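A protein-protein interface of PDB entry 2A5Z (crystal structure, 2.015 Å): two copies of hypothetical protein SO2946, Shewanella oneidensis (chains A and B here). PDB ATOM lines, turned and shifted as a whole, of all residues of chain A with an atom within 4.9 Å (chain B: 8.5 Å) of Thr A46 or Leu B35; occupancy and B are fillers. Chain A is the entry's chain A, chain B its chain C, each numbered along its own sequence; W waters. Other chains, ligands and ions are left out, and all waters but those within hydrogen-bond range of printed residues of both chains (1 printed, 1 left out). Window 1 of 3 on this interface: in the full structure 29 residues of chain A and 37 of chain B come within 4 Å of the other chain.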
ATOM      1  N   ILE A  44      17.481  16.601  -1.050  1.00  0.00           N
ATOM      2  CA  ILE A  44      16.697  17.560  -0.263  1.00  0.00           C
ATOM      3  C   ILE A  44      15.353  16.923   0.047  1.00  0.00           C
ATOM      4  O   ILE A  44      14.616  16.554  -0.869  1.00  0.00           O
ATOM      5  CB  ILE A  44      16.445  18.898  -1.009  1.00  0.00           C
ATOM      6  CG1 ILE A  44      17.751  19.496  -1.513  1.00  0.00           C
ATOM      7  CG2 ILE A  44      15.728  19.905  -0.082  1.00  0.00           C
ATOM      8  CD1 ILE A  44      17.616  20.877  -2.099  1.00  0.00           C
ATOM      9  N   ALA A  45      15.034  16.792   1.333  1.00  0.00           N
ATOM     10  CA  ALA A  45      13.769  16.194   1.733  1.00  0.00           C
ATOM     11  C   ALA A  45      12.624  17.186   1.576  1.00  0.00           C
ATOM     12  O   ALA A  45      12.793  18.386   1.818  1.00  0.00           O
ATOM     13  CB  ALA A  45      13.842  15.693   3.156  1.00  0.00           C
ATOM     14  N   THR A  46      11.470  16.682   1.151  1.00  0.00           N
ATOM     15  CA  THR A  46      10.233  17.462   1.189  1.00  0.00           C
ATOM     16  C   THR A  46       9.158  16.705   1.971  1.00  0.00           C
ATOM     17  O   THR A  46       8.872  17.057   3.113  1.00  0.00           O
ATOM     18  CB  THR A  46       9.739  17.884  -0.223  1.00  0.00           C
ATOM     19  OG1 THR A  46      10.761  18.644  -0.881  1.00  0.00           O
ATOM     20  CG2 THR A  46       8.483  18.755  -0.117  1.00  0.00           C
ATOM     21  N   SER A  47       8.595  15.656   1.373  1.00  0.00           N
ATOM     22  CA  SER A  47       7.481  14.911   1.980  1.00  0.00           C
ATOM     23  C   SER A  47       7.900  13.556   2.552  1.00  0.00           C
ATOM     24  O   SER A  47       7.267  13.028   3.468  1.00  0.00           O
ATOM     25  CB  SER A  47       6.377  14.697   0.948  1.00  0.00           C
ATOM     26  OG  SER A  47       6.796  13.770  -0.042  1.00  0.00           O
ATOM     27  N   ASP A  48       8.958  12.981   1.994  1.00  0.00           N
ATOM     28  CA  ASP A  48       9.380  11.644   2.398  1.00  0.00           C
ATOM     29  C   ASP A  48      10.894  11.511   2.413  1.00  0.00           C
ATOM     30  O   ASP A  48      11.618  12.397   1.946  1.00  0.00           O
ATOM     31  CB  ASP A  48       8.749  10.575   1.490  1.00  0.00           C
ATOM     32  CG  ASP A  48       9.046  10.809   0.018  1.00  0.00           C
ATOM     33  OD1 ASP A  48      10.222  11.060  -0.320  1.00  0.00           O
ATOM     34  OD2 ASP A  48       8.108  10.745  -0.809  1.00  0.00           O
ATOM     35  N   VAL A 255       8.349  12.479   6.134  1.00  0.00           N
ATOM     36  CA  VAL A 255       9.085  13.648   6.598  1.00  0.00           C
ATOM     37  C   VAL A 255       8.246  14.910   6.388  1.00  0.00           C
ATOM     38  O   VAL A 255       7.563  15.044   5.373  1.00  0.00           O
ATOM     39  CB  VAL A 255      10.452  13.776   5.843  1.00  0.00           C
ATOM     40  CG1 VAL A 255      11.117  15.104   6.133  1.00  0.00           C
ATOM     41  CG2 VAL A 255      11.392  12.633   6.213  1.00  0.00           C
ATOM     42  N   SER A 256       8.281  15.822   7.354  1.00  0.00           N
ATOM     43  CA  SER A 256       7.718  17.162   7.150  1.00  0.00           C
ATOM     44  C   SER A 256       8.872  18.159   6.988  1.00  0.00           C
ATOM     45  O   SER A 256       9.421  18.646   7.979  1.00  0.00           O
ATOM     46  CB  SER A 256       6.782  17.562   8.305  1.00  0.00           C
ATOM     47  OG  SER A 256       7.473  17.590   9.543  1.00  0.00           O
ATOM     48  N   ALA A 257       9.250  18.433   5.738  1.00  0.00           N
ATOM     49  CA  ALA A 257      10.442  19.236   5.451  1.00  0.00           C
ATOM     50  C   ALA A 257      10.210  20.306   4.382  1.00  0.00           C
ATOM     51  O   ALA A 257      10.924  20.362   3.374  1.00  0.00           O
ATOM     52  CB  ALA A 257      11.607  18.340   5.069  1.00  0.00           C
ATOM     53  N   THR A 258       9.228  21.167   4.624  1.00  0.00           N
ATOM     54  CA  THR A 258       8.917  22.267   3.721  1.00  0.00           C
ATOM     55  C   THR A 258       9.699  23.534   4.077  1.00  0.00           C
ATOM     56  O   THR A 258       9.393  24.199   5.074  1.00  0.00           O
ATOM     57  CB  THR A 258       7.412  22.599   3.767  1.00  0.00           C
ATOM     58  OG1 THR A 258       6.658  21.388   3.906  1.00  0.00           O
ATOM     59  CG2 THR A 258       6.982  23.331   2.509  1.00  0.00           C
ATOM     60  N   LYS A 261      11.331  28.510  -0.773  1.00  0.00           N
ATOM     61  CA  LYS A 261      12.135  28.553  -1.978  1.00  0.00           C
ATOM     62  C   LYS A 261      12.520  30.008  -2.174  1.00  0.00           C
ATOM     63  O   LYS A 261      11.735  30.908  -1.855  1.00  0.00           O
ATOM     64  CB  LYS A 261      11.322  28.062  -3.180  1.00  0.00           C
ATOM     65  CG  LYS A 261      10.800  26.626  -3.077  1.00  0.00           C
ATOM     66  CD  LYS A 261      11.828  25.604  -3.572  1.00  0.00           C
ATOM     67  CE  LYS A 261      11.202  24.218  -3.777  1.00  0.00           C
ATOM     68  NZ  LYS A 261      10.757  23.571  -2.494  1.00  0.00           N
ATOM     69  N   MET B  29       3.760  12.451 -15.337  1.00  0.00           N
ATOM     70  CA  MET B  29       4.631  12.609 -14.181  1.00  0.00           C
ATOM     71  C   MET B  29       3.967  13.537 -13.163  1.00  0.00           C
ATOM     72  O   MET B  29       3.503  14.625 -13.523  1.00  0.00           O
ATOM     73  CB  MET B  29       5.966  13.194 -14.650  1.00  0.00           C
ATOM     74  CG  MET B  29       7.086  13.192 -13.618  1.00  0.00           C
ATOM     75  SD  MET B  29       8.591  13.976 -14.235  1.00  0.00           S
ATOM     76  CE  MET B  29       8.042  15.655 -14.449  1.00  0.00           C
ATOM     77  N   SER B  30       3.919  13.099 -11.905  1.00  0.00           N
ATOM     78  CA  SER B  30       3.325  13.874 -10.803  1.00  0.00           C
ATOM     79  C   SER B  30       4.238  15.016 -10.332  1.00  0.00           C
ATOM     80  O   SER B  30       5.438  14.988 -10.599  1.00  0.00           O
ATOM     81  CB  SER B  30       2.983  12.952  -9.627  1.00  0.00           C
ATOM     82  OG  SER B  30       4.157  12.478  -8.983  1.00  0.00           O
ATOM     83  N   PRO B  31       3.668  16.029  -9.636  1.00  0.00           N
ATOM     84  CA  PRO B  31       4.468  17.131  -9.073  1.00  0.00           C
ATOM     85  C   PRO B  31       5.576  16.662  -8.121  1.00  0.00           C
ATOM     86  O   PRO B  31       6.668  17.230  -8.118  1.00  0.00           O
ATOM     87  CB  PRO B  31       3.426  17.970  -8.321  1.00  0.00           C
ATOM     88  CG  PRO B  31       2.137  17.674  -9.021  1.00  0.00           C
ATOM     89  CD  PRO B  31       2.228  16.221  -9.370  1.00  0.00           C
ATOM     90  N   SER B  32       5.288  15.627  -7.333  1.00  0.00           N
ATOM     91  CA  SER B  32       6.247  15.039  -6.398  1.00  0.00           C
ATOM     92  C   SER B  32       7.454  14.394  -7.110  1.00  0.00           C
ATOM     93  O   SER B  32       8.585  14.450  -6.615  1.00  0.00           O
ATOM     94  CB  SER B  32       5.540  14.009  -5.518  1.00  0.00           C
ATOM     95  OG  SER B  32       6.471  13.133  -4.906  1.00  0.00           O
ATOM     96  N   GLU B  33       7.197  13.778  -8.260  1.00  0.00           N
ATOM     97  CA  GLU B  33       8.253  13.185  -9.076  1.00  0.00           C
ATOM     98  C   GLU B  33       9.065  14.271  -9.790  1.00  0.00           C
ATOM     99  O   GLU B  33      10.277  14.130  -9.970  1.00  0.00           O
ATOM    100  CB  GLU B  33       7.663  12.174 -10.069  1.00  0.00           C
ATOM    101  CG  GLU B  33       7.158  10.879  -9.412  1.00  0.00           C
ATOM    102  CD  GLU B  33       6.140  10.101 -10.259  1.00  0.00           C
ATOM    103  OE1 GLU B  33       5.441  10.707 -11.102  1.00  0.00           O
ATOM    104  OE2 GLU B  33       6.029   8.870 -10.064  1.00  0.00           O
ATOM    105  N   LYS B  34       8.397  15.353 -10.185  1.00  0.00           N
ATOM    106  CA  LYS B  34       9.063  16.485 -10.839  1.00  0.00           C
ATOM    107  C   LYS B  34      10.033  17.163  -9.874  1.00  0.00           C
ATOM    108  O   LYS B  34      11.161  17.488 -10.245  1.00  0.00           O
ATOM    109  CB  LYS B  34       8.042  17.498 -11.381  1.00  0.00           C
ATOM    110  CG  LYS B  34       8.662  18.665 -12.161  1.00  0.00           C
ATOM    111  CD  LYS B  34       7.597  19.546 -12.815  1.00  0.00           C
ATOM    112  CE  LYS B  34       8.212  20.740 -13.547  1.00  0.00           C
ATOM    113  NZ  LYS B  34       8.953  20.350 -14.791  1.00  0.00           N
ATOM    114  N   LEU B  35       9.581  17.360  -8.636  1.00  0.00           N
ATOM    115  CA  LEU B  35      10.399  17.950  -7.577  1.00  0.00           C
ATOM    116  C   LEU B  35      11.634  17.103  -7.268  1.00  0.00           C
ATOM    117  O   LEU B  35      12.739  17.635  -7.215  1.00  0.00           O
ATOM    118  CB  LEU B  35       9.556  18.178  -6.315  1.00  0.00           C
ATOM    119  CG  LEU B  35      10.120  19.026  -5.167  1.00  0.00           C
ATOM    120  CD1 LEU B  35      10.488  20.458  -5.592  1.00  0.00           C
ATOM    121  CD2 LEU B  35       9.115  19.046  -4.014  1.00  0.00           C
ATOM    122  N   LYS B  36      11.435  15.797  -7.065  1.00  0.00           N
ATOM    123  CA  LYS B  36      12.518  14.821  -6.868  1.00  0.00           C
ATOM    124  C   LYS B  36      13.603  14.946  -7.922  1.00  0.00           C
ATOM    125  O   LYS B  36      14.790  14.952  -7.611  1.00  0.00           O
ATOM    126  CB  LYS B  36      11.973  13.392  -6.941  1.00  0.00           C
ATOM    127  CG  LYS B  36      11.606  12.758  -5.625  1.00  0.00           C
ATOM    128  CD  LYS B  36      11.547  11.247  -5.785  1.00  0.00           C
ATOM    129  CE  LYS B  36      10.808  10.606  -4.635  1.00  0.00           C
ATOM    130  NZ  LYS B  36      10.749   9.133  -4.794  1.00  0.00           N
ATOM    131  N   LEU B  37      13.177  15.024  -9.177  1.00  0.00           N
ATOM    132  CA  LEU B  37      14.089  15.097 -10.297  1.00  0.00           C
ATOM    133  C   LEU B  37      14.819  16.444 -10.338  1.00  0.00           C
ATOM    134  O   LEU B  37      15.979  16.511 -10.754  1.00  0.00           O
ATOM    135  CB  LEU B  37      13.325  14.815 -11.596  1.00  0.00           C
ATOM    136  CG  LEU B  37      14.013  14.047 -12.729  1.00  0.00           C
ATOM    137  CD1 LEU B  37      15.007  12.999 -12.237  1.00  0.00           C
ATOM    138  CD2 LEU B  37      12.960  13.398 -13.608  1.00  0.00           C
ATOM    139  N   SER B  38      14.153  17.502  -9.869  1.00  0.00           N
ATOM    140  CA  SER B  38      14.739  18.843  -9.853  1.00  0.00           C
ATOM    141  C   SER B  38      15.926  18.969  -8.894  1.00  0.00           C
ATOM    142  O   SER B  38      16.760  19.866  -9.034  1.00  0.00           O
ATOM    143  CB  SER B  38      13.676  19.901  -9.523  1.00  0.00           C
ATOM    144  OG  SER B  38      13.329  19.889  -8.143  1.00  0.00           O
ATOM    145  N   THR B  39      15.998  18.073  -7.918  1.00  0.00           N
ATOM    146  CA  THR B  39      17.056  18.127  -6.916  1.00  0.00           C
ATOM    147  C   THR B  39      18.046  16.960  -7.034  1.00  0.00           C
ATOM    148  O   THR B  39      18.836  16.709  -6.122  1.00  0.00           O
ATOM    149  CB  THR B  39      16.473  18.238  -5.487  1.00  0.00           C
ATOM    150  OG1 THR B  39      15.675  17.087  -5.204  1.00  0.00           O
ATOM    151  CG2 THR B  39      15.618  19.505  -5.342  1.00  0.00           C
ATOM    152  N   LEU B  40      18.012  16.271  -8.174  1.00  0.00           N
ATOM    153  CA  LEU B  40      18.941  15.179  -8.467  1.00  0.00           C
ATOM    154  C   LEU B  40      20.381  15.674  -8.643  1.00  0.00           C
ATOM    155  O   LEU B  40      20.647  16.596  -9.416  1.00  0.00           O
ATOM    156  CB  LEU B  40      18.468  14.390  -9.697  1.00  0.00           C
ATOM    157  CG  LEU B  40      19.390  13.335 -10.323  1.00  0.00           C
ATOM    158  CD1 LEU B  40      19.652  12.194  -9.365  1.00  0.00           C
ATOM    159  CD2 LEU B  40      18.799  12.812 -11.618  1.00  0.00           C
ATOM    160  N   TYR B  50      23.984  20.432 -10.674  1.00  0.00           N
ATOM    161  CA  TYR B  50      23.240  20.534  -9.428  1.00  0.00           C
ATOM    162  C   TYR B  50      23.847  19.642  -8.343  1.00  0.00           C
ATOM    163  O   TYR B  50      24.216  18.500  -8.613  1.00  0.00           O
ATOM    164  CB  TYR B  50      21.766  20.155  -9.642  1.00  0.00           C
ATOM    165  CG  TYR B  50      20.923  20.492  -8.443  1.00  0.00           C
ATOM    166  CD1 TYR B  50      20.350  21.758  -8.311  1.00  0.00           C
ATOM    167  CD2 TYR B  50      20.732  19.567  -7.416  1.00  0.00           C
ATOM    168  CE1 TYR B  50      19.586  22.091  -7.192  1.00  0.00           C
ATOM    169  CE2 TYR B  50      19.976  19.897  -6.282  1.00  0.00           C
ATOM    170  CZ  TYR B  50      19.415  21.154  -6.185  1.00  0.00           C
ATOM    171  OH  TYR B  50      18.665  21.483  -5.088  1.00  0.00           O
ATOM    172  N   ASP B  54      21.573  17.828   2.796  1.00  0.00           N
ATOM    173  CA  ASP B  54      20.573  18.197   3.798  1.00  0.00           C
ATOM    174  C   ASP B  54      20.986  17.820   5.229  1.00  0.00           C
ATOM    175  O   ASP B  54      20.167  17.864   6.137  1.00  0.00           O
ATOM    176  CB  ASP B  54      19.218  17.545   3.450  1.00  0.00           C
ATOM    177  CG  ASP B  54      18.015  18.391   3.869  1.00  0.00           C
ATOM    178  OD1 ASP B  54      18.182  19.411   4.559  1.00  0.00           O
ATOM    179  OD2 ASP B  54      16.869  18.045   3.495  1.00  0.00           O
ATOM    180  N   ASN B  86      10.506  22.241  10.145  1.00  0.00           N
ATOM    181  CA  ASN B  86      10.669  21.801   8.766  1.00  0.00           C
ATOM    182  C   ASN B  86      12.131  21.639   8.357  1.00  0.00           C
ATOM    183  O   ASN B  86      12.427  21.240   7.226  1.00  0.00           O
ATOM    184  CB  ASN B  86       9.950  22.765   7.827  1.00  0.00           C
ATOM    185  CG  ASN B  86       8.455  22.522   7.788  1.00  0.00           C
ATOM    186  OD1 ASN B  86       7.989  21.556   7.187  1.00  0.00           O
ATOM    187  ND2 ASN B  86       7.696  23.395   8.435  1.00  0.00           N
ATOM    188  N   PHE B  88      14.925  19.571   8.290  1.00  0.00           N
ATOM    189  CA  PHE B  88      15.234  18.148   8.390  1.00  0.00           C
ATOM    190  C   PHE B  88      16.738  17.965   8.267  1.00  0.00           C
ATOM    191  O   PHE B  88      17.299  18.282   7.234  1.00  0.00           O
ATOM    192  CB  PHE B  88      14.532  17.404   7.249  1.00  0.00           C
ATOM    193  CG  PHE B  88      14.887  15.944   7.140  1.00  0.00           C
ATOM    194  CD1 PHE B  88      14.346  15.011   8.022  1.00  0.00           C
ATOM    195  CD2 PHE B  88      15.731  15.493   6.132  1.00  0.00           C
ATOM    196  CE1 PHE B  88      14.662  13.659   7.914  1.00  0.00           C
ATOM    197  CE2 PHE B  88      16.054  14.137   6.016  1.00  0.00           C
ATOM    198  CZ  PHE B  88      15.518  13.221   6.911  1.00  0.00           C
ATOM    199  N   LEU B 248      20.938  22.945   5.278  1.00  0.00           N
ATOM    200  CA  LEU B 248      20.838  22.635   3.863  1.00  0.00           C
ATOM    201  C   LEU B 248      21.706  23.578   3.043  1.00  0.00           C
ATOM    202  O   LEU B 248      21.745  24.783   3.306  1.00  0.00           O
ATOM    203  CB  LEU B 248      19.364  22.752   3.431  1.00  0.00           C
ATOM    204  CG  LEU B 248      18.885  22.648   1.978  1.00  0.00           C
ATOM    205  CD1 LEU B 248      19.322  21.344   1.349  1.00  0.00           C
ATOM    206  CD2 LEU B 248      17.370  22.774   1.926  1.00  0.00           C
HETATM  207  O   HOH W   1      16.961  15.477   2.697  1.00  0.00           O
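The backbone NH (N) of Ala A257 is in hydrogen-bond range of the backbone carbonyl oxygen (O) of Thr A46 (3.0 Å).
O of Ser A47 is in hydrogen-bond range of N of Val A255, at 2.9 Å.
The backbone carbonyl oxygen (O) of Leu B35 lies within hydrogen-bond range of the side-chain hydroxyl (OG) of Ser B38 (2.5 Å).
Hydrophobic or aromatic side chains of chain B within 4 Å of the printed part of chain A: Leu B35, Tyr B50, Phe B88 and Leu B248.
Of the 10 printed residues of chain A, 7 touch a printed residue of chain B.
Among the printed residues, 11 pairs touch across the chains.
Among the printed residues, no Asp or Glu carboxylate lies within 4 Å of a Lys or Arg side-chain nitrogen of the other chain.
Among the printed residues, pairs that only touch across the chains: Ile A44 with Tyr B50 (3.2 Å), Ile A44 with Asp B54 (3.8 Å), Ile A44 with Leu B248 (3.8 Å), Ala A45 with Phe B88 (3.5 Å), Thr A46 with Leu B35 (3.6 Å), Val A255 with Phe B88 (3.7 Å), Ala A257 with Asn B86 (3.3 Å) and Ala A257 with Phe B88 (3.8 Å).
No position is printed for both chains.
Of the 11 pairs that touch across the chains among the printed residues, none has its exchanged pair printed and touching as well.
Ala A45 touches two residues of chain B.
Printed residues of chain B within 4 Å of Thr A46: Leu B35.
No residue of chain B comes within 4 Å of Ser A47.
Of the printed residues of chain B, Val A255 touches Phe B88 (3.7 Å).
Of the printed residues of chain B, Ser A256 touches Asn B86 (3.3 Å).
Of chain B, only Asn B86 and Phe B88 come within 4 Å of Ala A257.
Of chain A, only Thr A46 (3.6 Å) comes within 4 Å of Leu B35.
Printed residues of chain A within 4 Å of Asp B54: Ile A44 and Ala A45.
Of the printed residues of chain A, Phe B88 touches Ala A45, Val A255 and Ala A257.
Of the printed residues of chain A, Leu B248 touches Ile A44.
The nearest residue of chain B that does not touch Thr A46 is Asp B54 (6.0 Å).
The nearest residue of chain A that does not touch Leu B35 is Lys A261 (4.2 Å).
The nearest printed residue of chain B that does not touch Ile A44 is Thr B39 (4.05 Å).
The side-chain carboxylate (OD2) of Asp B54 lies within hydrogen-bond range of the backbone NH (N) of Ala A45.
The backbone NH (N) of Thr A258 lies within hydrogen-bond range of the side-chain amide oxygen (OD1) of Asn B86 (2.9 Å).
OD1 of Asn B86 lies close to O of Ser A256 (3.3 Å).
Water W1 lies within hydrogen-bond range of the side-chain carboxylate of Asp B54 (2.7 Å) and the backbone NH of Ala A45 (2.7 Å).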
